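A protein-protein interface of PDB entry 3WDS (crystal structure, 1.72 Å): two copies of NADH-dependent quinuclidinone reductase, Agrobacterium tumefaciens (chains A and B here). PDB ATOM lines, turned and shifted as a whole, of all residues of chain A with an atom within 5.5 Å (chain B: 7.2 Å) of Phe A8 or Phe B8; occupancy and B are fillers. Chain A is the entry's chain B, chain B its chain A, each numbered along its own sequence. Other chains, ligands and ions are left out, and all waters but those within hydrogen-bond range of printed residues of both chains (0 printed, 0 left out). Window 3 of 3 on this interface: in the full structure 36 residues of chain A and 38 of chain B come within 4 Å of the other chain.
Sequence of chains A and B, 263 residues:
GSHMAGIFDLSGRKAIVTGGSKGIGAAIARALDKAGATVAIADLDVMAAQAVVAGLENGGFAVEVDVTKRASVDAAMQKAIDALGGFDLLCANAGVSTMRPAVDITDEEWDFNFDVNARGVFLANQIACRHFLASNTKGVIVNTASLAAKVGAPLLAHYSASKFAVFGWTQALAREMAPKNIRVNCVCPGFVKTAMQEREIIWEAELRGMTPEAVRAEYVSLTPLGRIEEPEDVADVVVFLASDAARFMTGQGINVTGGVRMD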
ATOM      1  N   ILE A   7      12.077 -21.338   0.558  1.00  0.00           N
ATOM      2  CA  ILE A   7      11.697 -22.788   0.461  1.00  0.00           C
ATOM      3  C   ILE A   7      12.321 -23.663   1.565  1.00  0.00           C
ATOM      4  O   ILE A   7      11.882 -24.825   1.738  1.00  0.00           O
ATOM      5  CB  ILE A   7      12.074 -23.344  -0.931  1.00  0.00           C
ATOM      6  CG1 ILE A   7      11.135 -24.539  -1.328  1.00  0.00           C
ATOM      7  CG2 ILE A   7      13.578 -23.547  -0.999  1.00  0.00           C
ATOM      8  CD1 ILE A   7       9.664 -24.151  -1.541  1.00  0.00           C
ATOM      9  N   PHE A   8      13.358 -23.209   2.246  1.00  0.00           N
ATOM     10  CA  PHE A   8      13.875 -23.995   3.403  1.00  0.00           C
ATOM     11  C   PHE A   8      13.203 -23.593   4.723  1.00  0.00           C
ATOM     12  O   PHE A   8      13.610 -24.090   5.782  1.00  0.00           O
ATOM     13  CB  PHE A   8      15.400 -23.991   3.543  1.00  0.00           C
ATOM     14  CG  PHE A   8      16.113 -24.442   2.290  1.00  0.00           C
ATOM     15  CD1 PHE A   8      16.260 -25.792   1.977  1.00  0.00           C
ATOM     16  CD2 PHE A   8      16.575 -23.509   1.398  1.00  0.00           C
ATOM     17  CE1 PHE A   8      16.850 -26.190   0.787  1.00  0.00           C
ATOM     18  CE2 PHE A   8      17.179 -23.891   0.196  1.00  0.00           C
ATOM     19  CZ  PHE A   8      17.274 -25.259  -0.123  1.00  0.00           C
ATOM     20  N   ASP A   9      12.230 -22.702   4.661  1.00  0.00           N
ATOM     21  CA  ASP A   9      11.607 -22.108   5.902  1.00  0.00           C
ATOM     22  C   ASP A   9      10.648 -23.112   6.513  1.00  0.00           C
ATOM     23  O   ASP A   9       9.810 -23.695   5.778  1.00  0.00           O
ATOM     24  CB  ASP A   9      10.810 -20.858   5.455  1.00  0.00           C
ATOM     25  CG  ASP A   9      10.301 -19.993   6.599  1.00  0.00           C
ATOM     26  OD1 ASP A   9      10.756 -20.137   7.716  1.00  0.00           O
ATOM     27  OD2 ASP A   9       9.472 -19.092   6.315  1.00  0.00           O
ATOM     28  N   LEU A  10      10.634 -23.199   7.868  1.00  0.00           N
ATOM     29  CA  LEU A  10       9.718 -24.054   8.621  1.00  0.00           C
ATOM     30  C   LEU A  10       8.791 -23.214   9.499  1.00  0.00           C
ATOM     31  O   LEU A  10       8.102 -23.702  10.387  1.00  0.00           O
ATOM     32  CB  LEU A  10      10.450 -25.096   9.474  1.00  0.00           C
ATOM     33  CG  LEU A  10      11.319 -26.107   8.706  1.00  0.00           C
ATOM     34  CD1 LEU A  10      11.934 -27.160   9.635  1.00  0.00           C
ATOM     35  CD2 LEU A  10      10.558 -26.775   7.612  1.00  0.00           C
ATOM     36  N   ALA A  35      15.044 -22.888  11.979  1.00  0.00           N
ATOM     37  CA  ALA A  35      14.358 -22.754  10.702  1.00  0.00           C
ATOM     38  C   ALA A  35      12.930 -22.271  10.780  1.00  0.00           C
ATOM     39  O   ALA A  35      12.267 -22.012   9.768  1.00  0.00           O
ATOM     40  CB  ALA A  35      14.416 -24.132   9.949  1.00  0.00           C
ATOM     41  N   ASP A 236      21.163 -30.473   9.940  1.00  0.00           N
ATOM     42  CA  ASP A 236      20.878 -29.501   8.914  1.00  0.00           C
ATOM     43  C   ASP A 236      20.243 -30.240   7.700  1.00  0.00           C
ATOM     44  O   ASP A 236      19.418 -29.695   6.972  1.00  0.00           O
ATOM     45  CB  ASP A 236      22.133 -28.738   8.530  1.00  0.00           C
ATOM     46  CG  ASP A 236      22.581 -27.768   9.620  1.00  0.00           C
ATOM     47  OD1 ASP A 236      21.728 -27.485  10.489  1.00  0.00           O
ATOM     48  OD2 ASP A 236      23.721 -27.304   9.554  1.00  0.00           O
ATOM     49  N   VAL A 239      16.493 -30.761   8.510  1.00  0.00           N
ATOM     50  CA  VAL A 239      15.797 -29.580   8.166  1.00  0.00           C
ATOM     51  C   VAL A 239      15.415 -29.548   6.675  1.00  0.00           C
ATOM     52  O   VAL A 239      14.238 -29.333   6.333  1.00  0.00           O
ATOM     53  CB  VAL A 239      16.574 -28.311   8.560  1.00  0.00           C
ATOM     54  CG1 VAL A 239      15.894 -27.136   7.943  1.00  0.00           C
ATOM     55  CG2 VAL A 239      16.770 -28.232  10.038  1.00  0.00           C
ATOM     56  N   PHE A 240      16.398 -29.824   5.803  1.00  0.00           N
ATOM     57  CA  PHE A 240      16.107 -29.973   4.411  1.00  0.00           C
ATOM     58  C   PHE A 240      14.927 -30.956   4.153  1.00  0.00           C
ATOM     59  O   PHE A 240      13.946 -30.637   3.448  1.00  0.00           O
ATOM     60  CB  PHE A 240      17.372 -30.413   3.691  1.00  0.00           C
ATOM     61  CG  PHE A 240      17.092 -30.936   2.307  1.00  0.00           C
ATOM     62  CD1 PHE A 240      16.547 -30.087   1.332  1.00  0.00           C
ATOM     63  CD2 PHE A 240      17.303 -32.234   2.054  1.00  0.00           C
ATOM     64  CE1 PHE A 240      16.269 -30.573   0.044  1.00  0.00           C
ATOM     65  CE2 PHE A 240      16.955 -32.763   0.803  1.00  0.00           C
ATOM     66  CZ  PHE A 240      16.470 -31.903  -0.192  1.00  0.00           C
ATOM     67  N   SER A 243      11.518 -29.770   4.977  1.00  0.00           N
ATOM     68  CA  SER A 243      11.116 -28.534   4.320  1.00  0.00           C
ATOM     69  C   SER A 243      10.532 -28.811   2.991  1.00  0.00           C
ATOM     70  O   SER A 243      10.606 -29.945   2.431  1.00  0.00           O
ATOM     71  CB  SER A 243      12.304 -27.605   4.096  1.00  0.00           C
ATOM     72  OG  SER A 243      13.077 -28.066   2.977  1.00  0.00           O
ATOM     73  N   ALA A 245      11.583 -27.846   0.274  1.00  0.00           N
ATOM     74  CA  ALA A 245      12.603 -28.073  -0.761  1.00  0.00           C
ATOM     75  C   ALA A 245      12.673 -29.548  -1.097  1.00  0.00           C
ATOM     76  O   ALA A 245      13.100 -29.905  -2.213  1.00  0.00           O
ATOM     77  CB  ALA A 245      13.971 -27.554  -0.345  1.00  0.00           C
ATOM     78  N   ILE B   7      22.298 -21.330   6.804  1.00  0.00           N
ATOM     79  CA  ILE B   7      23.117 -22.508   6.351  1.00  0.00           C
ATOM     80  C   ILE B   7      22.659 -22.861   4.896  1.00  0.00           C
ATOM     81  O   ILE B   7      23.358 -23.625   4.200  1.00  0.00           O
ATOM     82  CB  ILE B   7      22.944 -23.703   7.359  1.00  0.00           C
ATOM     83  CG1 ILE B   7      24.048 -24.765   7.221  1.00  0.00           C
ATOM     84  CG2 ILE B   7      21.574 -24.366   7.212  1.00  0.00           C
ATOM     85  CD1 ILE B   7      25.441 -24.172   7.347  1.00  0.00           C
ATOM     86  N   PHE B   8      21.501 -22.386   4.420  1.00  0.00           N
ATOM     87  CA  PHE B   8      21.107 -22.668   2.994  1.00  0.00           C
ATOM     88  C   PHE B   8      21.444 -21.539   2.021  1.00  0.00           C
ATOM     89  O   PHE B   8      21.160 -21.620   0.822  1.00  0.00           O
ATOM     90  CB  PHE B   8      19.634 -23.110   2.750  1.00  0.00           C
ATOM     91  CG  PHE B   8      19.192 -24.247   3.658  1.00  0.00           C
ATOM     92  CD1 PHE B   8      19.422 -25.566   3.310  1.00  0.00           C
ATOM     93  CD2 PHE B   8      18.668 -23.968   4.898  1.00  0.00           C
ATOM     94  CE1 PHE B   8      19.026 -26.585   4.162  1.00  0.00           C
ATOM     95  CE2 PHE B   8      18.278 -24.980   5.765  1.00  0.00           C
ATOM     96  CZ  PHE B   8      18.489 -26.309   5.412  1.00  0.00           C
ATOM     97  N   ASP B   9      22.121 -20.519   2.540  1.00  0.00           N
ATOM     98  CA  ASP B   9      22.363 -19.293   1.778  1.00  0.00           C
ATOM     99  C   ASP B   9      23.560 -19.513   0.849  1.00  0.00           C
ATOM    100  O   ASP B   9      24.566 -20.103   1.239  1.00  0.00           O
ATOM    101  CB  ASP B   9      22.725 -18.196   2.818  1.00  0.00           C
ATOM    102  CG  ASP B   9      22.940 -16.833   2.202  1.00  0.00           C
ATOM    103  OD1 ASP B   9      22.541 -16.580   1.074  1.00  0.00           O
ATOM    104  OD2 ASP B   9      23.506 -15.952   2.911  1.00  0.00           O
ATOM    105  N   LEU B  10      23.480 -19.011  -0.377  1.00  0.00           N
ATOM    106  CA  LEU B  10      24.580 -19.116  -1.324  1.00  0.00           C
ATOM    107  C   LEU B  10      25.048 -17.700  -1.685  1.00  0.00           C
ATOM    108  O   LEU B  10      25.784 -17.512  -2.655  1.00  0.00           O
ATOM    109  CB  LEU B  10      24.159 -19.863  -2.599  1.00  0.00           C
ATOM    110  CG  LEU B  10      23.614 -21.295  -2.440  1.00  0.00           C
ATOM    111  CD1 LEU B  10      23.282 -21.862  -3.806  1.00  0.00           C
ATOM    112  CD2 LEU B  10      24.688 -22.114  -1.783  1.00  0.00           C
ATOM    113  N   SER B  11      24.647 -16.729  -0.866  1.00  0.00           N
ATOM    114  CA  SER B  11      25.033 -15.297  -1.118  1.00  0.00           C
ATOM    115  C   SER B  11      26.535 -15.156  -1.358  1.00  0.00           C
ATOM    116  O   SER B  11      27.353 -15.731  -0.658  1.00  0.00           O
ATOM    117  CB  SER B  11      24.570 -14.376   0.024  1.00  0.00           C
ATOM    118  OG  SER B  11      23.166 -14.278   0.001  1.00  0.00           O
ATOM    119  N   ARG B  13      28.346 -16.426  -3.722  1.00  0.00           N
ATOM    120  CA  ARG B  13      29.016 -17.514  -4.385  1.00  0.00           C
ATOM    121  C   ARG B  13      28.856 -17.372  -5.859  1.00  0.00           C
ATOM    122  O   ARG B  13      27.869 -16.798  -6.338  1.00  0.00           O
ATOM    123  CB  ARG B  13      28.446 -18.827  -3.883  1.00  0.00           C
ATOM    124  CG  ARG B  13      28.755 -18.963  -2.407  1.00  0.00           C
ATOM    125  CD  ARG B  13      28.402 -20.300  -1.794  1.00  0.00           C
ATOM    126  NE  ARG B  13      28.448 -20.146  -0.346  1.00  0.00           N
ATOM    127  CZ  ARG B  13      28.438 -21.138   0.526  1.00  0.00           C
ATOM    128  NH1 ARG B  13      28.332 -22.404   0.102  1.00  0.00           N
ATOM    129  NH2 ARG B  13      28.479 -20.848   1.811  1.00  0.00           N
ATOM    130  N   ALA B  35      18.799 -18.075  -4.269  1.00  0.00           N
ATOM    131  CA  ALA B  35      19.478 -18.345  -3.047  1.00  0.00           C
ATOM    132  C   ALA B  35      20.665 -17.451  -2.793  1.00  0.00           C
ATOM    133  O   ALA B  35      21.314 -17.632  -1.771  1.00  0.00           O
ATOM    134  CB  ALA B  35      19.924 -19.814  -2.974  1.00  0.00           C
ATOM    135  N   GLY B  36      21.016 -16.573  -3.740  1.00  0.00           N
ATOM    136  CA  GLY B  36      22.063 -15.643  -3.477  1.00  0.00           C
ATOM    137  C   GLY B  36      23.278 -15.724  -4.351  1.00  0.00           C
ATOM    138  O   GLY B  36      24.103 -14.789  -4.405  1.00  0.00           O
ATOM    139  N   ALA B 235      15.390 -28.472  -8.933  1.00  0.00           N
ATOM    140  CA  ALA B 235      16.296 -27.350  -8.740  1.00  0.00           C
ATOM    141  C   ALA B 235      16.477 -27.052  -7.242  1.00  0.00           C
ATOM    142  O   ALA B 235      17.529 -26.744  -6.747  1.00  0.00           O
ATOM    143  CB  ALA B 235      15.671 -26.133  -9.437  1.00  0.00           C
ATOM    144  N   ASP B 236      15.383 -27.188  -6.503  1.00  0.00           N
ATOM    145  CA  ASP B 236      15.478 -26.860  -5.049  1.00  0.00           C
ATOM    146  C   ASP B 236      16.405 -27.851  -4.287  1.00  0.00           C
ATOM    147  O   ASP B 236      17.039 -27.497  -3.289  1.00  0.00           O
ATOM    148  CB  ASP B 236      14.105 -26.796  -4.478  1.00  0.00           C
ATOM    149  CG  ASP B 236      13.305 -25.529  -4.911  1.00  0.00           C
ATOM    150  OD1 ASP B 236      13.893 -24.604  -5.560  1.00  0.00           O
ATOM    151  OD2 ASP B 236      12.053 -25.506  -4.642  1.00  0.00           O
ATOM    152  N   VAL B 237      16.455 -29.106  -4.714  1.00  0.00           N
ATOM    153  CA  VAL B 237      17.345 -30.078  -4.133  1.00  0.00           C
ATOM    154  C   VAL B 237      18.776 -29.774  -4.544  1.00  0.00           C
ATOM    155  O   VAL B 237      19.732 -29.965  -3.730  1.00  0.00           O
ATOM    156  CB  VAL B 237      16.919 -31.515  -4.521  1.00  0.00           C
ATOM    157  CG1 VAL B 237      17.897 -32.539  -3.955  1.00  0.00           C
ATOM    158  CG2 VAL B 237      15.454 -31.736  -4.124  1.00  0.00           C
ATOM    159  N   VAL B 238      18.964 -29.328  -5.763  1.00  0.00           N
ATOM    160  CA  VAL B 238      20.291 -28.874  -6.218  1.00  0.00           C
ATOM    161  C   VAL B 238      20.794 -27.731  -5.314  1.00  0.00           C
ATOM    162  O   VAL B 238      21.991 -27.702  -4.903  1.00  0.00           O
ATOM    163  CB  VAL B 238      20.343 -28.463  -7.692  1.00  0.00           C
ATOM    164  CG1 VAL B 238      21.690 -27.876  -8.114  1.00  0.00           C
ATOM    165  CG2 VAL B 238      20.047 -29.680  -8.557  1.00  0.00           C
ATOM    166  N   VAL B 239      19.922 -26.758  -5.048  1.00  0.00           N
ATOM    167  CA  VAL B 239      20.262 -25.721  -4.098  1.00  0.00           C
ATOM    168  C   VAL B 239      20.755 -26.285  -2.776  1.00  0.00           C
ATOM    169  O   VAL B 239      21.839 -25.894  -2.255  1.00  0.00           O
ATOM    170  CB  VAL B 239      19.121 -24.717  -3.869  1.00  0.00           C
ATOM    171  CG1 VAL B 239      19.487 -23.764  -2.772  1.00  0.00           C
ATOM    172  CG2 VAL B 239      18.890 -23.939  -5.160  1.00  0.00           C
ATOM    173  N   PHE B 240      19.979 -27.217  -2.196  1.00  0.00           N
ATOM    174  CA  PHE B 240      20.416 -27.839  -0.999  1.00  0.00           C
ATOM    175  C   PHE B 240      21.797 -28.486  -1.158  1.00  0.00           C
ATOM    176  O   PHE B 240      22.664 -28.303  -0.297  1.00  0.00           O
ATOM    177  CB  PHE B 240      19.363 -28.938  -0.555  1.00  0.00           C
ATOM    178  CG  PHE B 240      19.945 -29.933   0.405  1.00  0.00           C
ATOM    179  CD1 PHE B 240      20.292 -29.537   1.646  1.00  0.00           C
ATOM    180  CD2 PHE B 240      20.140 -31.273   0.063  1.00  0.00           C
ATOM    181  CE1 PHE B 240      20.809 -30.435   2.553  1.00  0.00           C
ATOM    182  CE2 PHE B 240      20.692 -32.160   0.974  1.00  0.00           C
ATOM    183  CZ  PHE B 240      21.014 -31.724   2.216  1.00  0.00           C
ATOM    184  N   LEU B 241      22.044 -29.312  -2.191  1.00  0.00           N
ATOM    185  CA  LEU B 241      23.331 -29.954  -2.342  1.00  0.00           C
ATOM    186  C   LEU B 241      24.514 -29.013  -2.528  1.00  0.00           C
ATOM    187  O   LEU B 241      25.626 -29.359  -2.175  1.00  0.00           O
ATOM    188  CB  LEU B 241      23.317 -30.970  -3.494  1.00  0.00           C
ATOM    189  CG  LEU B 241      22.417 -32.171  -3.230  1.00  0.00           C
ATOM    190  CD1 LEU B 241      22.238 -32.997  -4.496  1.00  0.00           C
ATOM    191  CD2 LEU B 241      23.045 -33.063  -2.168  1.00  0.00           C
ATOM    192  N   ALA B 242      24.246 -27.877  -3.094  1.00  0.00           N
ATOM    193  CA  ALA B 242      25.255 -26.798  -3.314  1.00  0.00           C
ATOM    194  C   ALA B 242      25.654 -26.170  -1.983  1.00  0.00           C
ATOM    195  O   ALA B 242      26.746 -25.647  -1.833  1.00  0.00           O
ATOM    196  CB  ALA B 242      24.694 -25.764  -4.216  1.00  0.00           C
ATOM    197  N   SER B 243      24.696 -26.158  -1.069  1.00  0.00           N
ATOM    198  CA  SER B 243      24.735 -25.386   0.181  1.00  0.00           C
ATOM    199  C   SER B 243      25.539 -26.081   1.259  1.00  0.00           C
ATOM    200  O   SER B 243      25.790 -27.300   1.239  1.00  0.00           O
ATOM    201  CB  SER B 243      23.365 -25.063   0.746  1.00  0.00           C
ATOM    202  OG  SER B 243      22.762 -26.171   1.422  1.00  0.00           O
ATOM    203  N   ASP B 244      25.857 -25.322   2.293  1.00  0.00           N
ATOM    204  CA  ASP B 244      26.629 -25.883   3.387  1.00  0.00           C
ATOM    205  C   ASP B 244      25.808 -26.802   4.302  1.00  0.00           C
ATOM    206  O   ASP B 244      26.368 -27.469   5.180  1.00  0.00           O
ATOM    207  CB  ASP B 244      27.264 -24.753   4.212  1.00  0.00           C
ATOM    208  CG  ASP B 244      28.268 -23.948   3.446  1.00  0.00           C
ATOM    209  OD1 ASP B 244      28.720 -24.254   2.325  1.00  0.00           O
ATOM    210  OD2 ASP B 244      28.654 -22.891   4.055  1.00  0.00           O
ATOM    211  N   ALA B 245      24.477 -26.829   4.063  1.00  0.00           N
ATOM    212  CA  ALA B 245      23.590 -27.757   4.759  1.00  0.00           C
ATOM    213  C   ALA B 245      24.012 -29.207   4.387  1.00  0.00           C
ATOM    214  O   ALA B 245      23.832 -30.158   5.220  1.00  0.00           O
ATOM    215  CB  ALA B 245      22.130 -27.537   4.501  1.00  0.00           C
ATOM    216  N   ALA B 246      24.595 -29.311   3.214  1.00  0.00           N
ATOM    217  CA  ALA B 246      25.074 -30.606   2.689  1.00  0.00           C
ATOM    218  C   ALA B 246      26.580 -30.820   2.835  1.00  0.00           C
ATOM    219  O   ALA B 246      27.182 -31.617   2.145  1.00  0.00           O
ATOM    220  CB  ALA B 246      24.571 -30.841   1.240  1.00  0.00           C
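Of the 10 printed residues of chain A, 6 touch a printed residue of chain B. Hydrophobic or aromatic side chains of chain A within 4 Å of the printed part of chain B: Ile A7, Phe A8, Val A239 and Phe A240. Along chain A the printed residues that touch a printed residue of chain B span positions 7 to 245. Of the 20 printed residues of chain B, 7 touch a printed residue of chain A. Hydrophobic or aromatic side chains of chain B that line the printed part of chain A: Ile B7, Phe B8, Val B237, Val B239 and Phe B240. Among the printed residues, 12 pairs touch across the chains. Among the printed residues, no Asp or Glu carboxylate lies within 4 Å of a Lys or Arg side-chain nitrogen of the other chain.
Phe A8 touches four residues of chain B. Printed residues of chain B within 4 Å of Ala A245: Asp B236 (3.98 Å) and Val B237 (3.5 Å). Phe B8 touches three residues of chain A. Gly B36 touches none of the printed residues of chain A. Printed residues of chain A within 4 Å of Phe B240: Phe A8 and Phe A240. The nearest residue of chain A that does not touch Phe B8 is Phe A240 (4.1 Å).
Asp B236 touches Ile A7. CD2 of Phe A8 touches CB of Phe B8 (3.4 Å). Asp B236 touches Phe A8 (O to CZ, 3.9 Å). Phe A8 touches Val B239. N of Phe B240 touches CZ of Phe A8, 3.9 Å away. Asp A236 touches Phe B8 (O to CZ, 3.8 Å). CB of Asp A236 touches O of Ala B245, 3.98 Å away. Val A239 touches Phe B8. O of Ala A245 touches CB of Asp B236 (3.98 Å). O of Ala A245 touches CG2 of Val B237, at 3.5 Å.
Ile A7 touches Asp B236, and with the chains exchanged Asp A236 touches Ile B7. Phe A8 touches Phe B240, but with the chains exchanged Phe A240 does not touch Phe B8 (4.1 Å). Asp A236 touches Ala B245, and with the chains exchanged Ala A245 touches Asp B236. Phe A240 touches its own counterpart, Phe B240. 10 positions are printed for both chains.
The backbone carbonyl oxygen of Ile B7 sits at hydrogen-bond distance from the backbone NH of Ala B245. The backbone carbonyl oxygen (O) of Phe B240 sits at hydrogen-bond distance from the side-chain hydroxyl (OG) of Ser B243. OG of Ser B243 lies close to N of Ala B245, at 3.2 Å. N of Ala A245 lies within hydrogen-bond range of O of Ile A7, at 3.4 Å. The backbone carbonyl oxygen (O) of Phe A240 sits at hydrogen-bond distance from the side-chain hydroxyl (OG) of Ser A243 (2.8 Å). The side-chain hydroxyl of Ser A243 sits close to the backbone NH of Ala A245 (3.1 Å).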
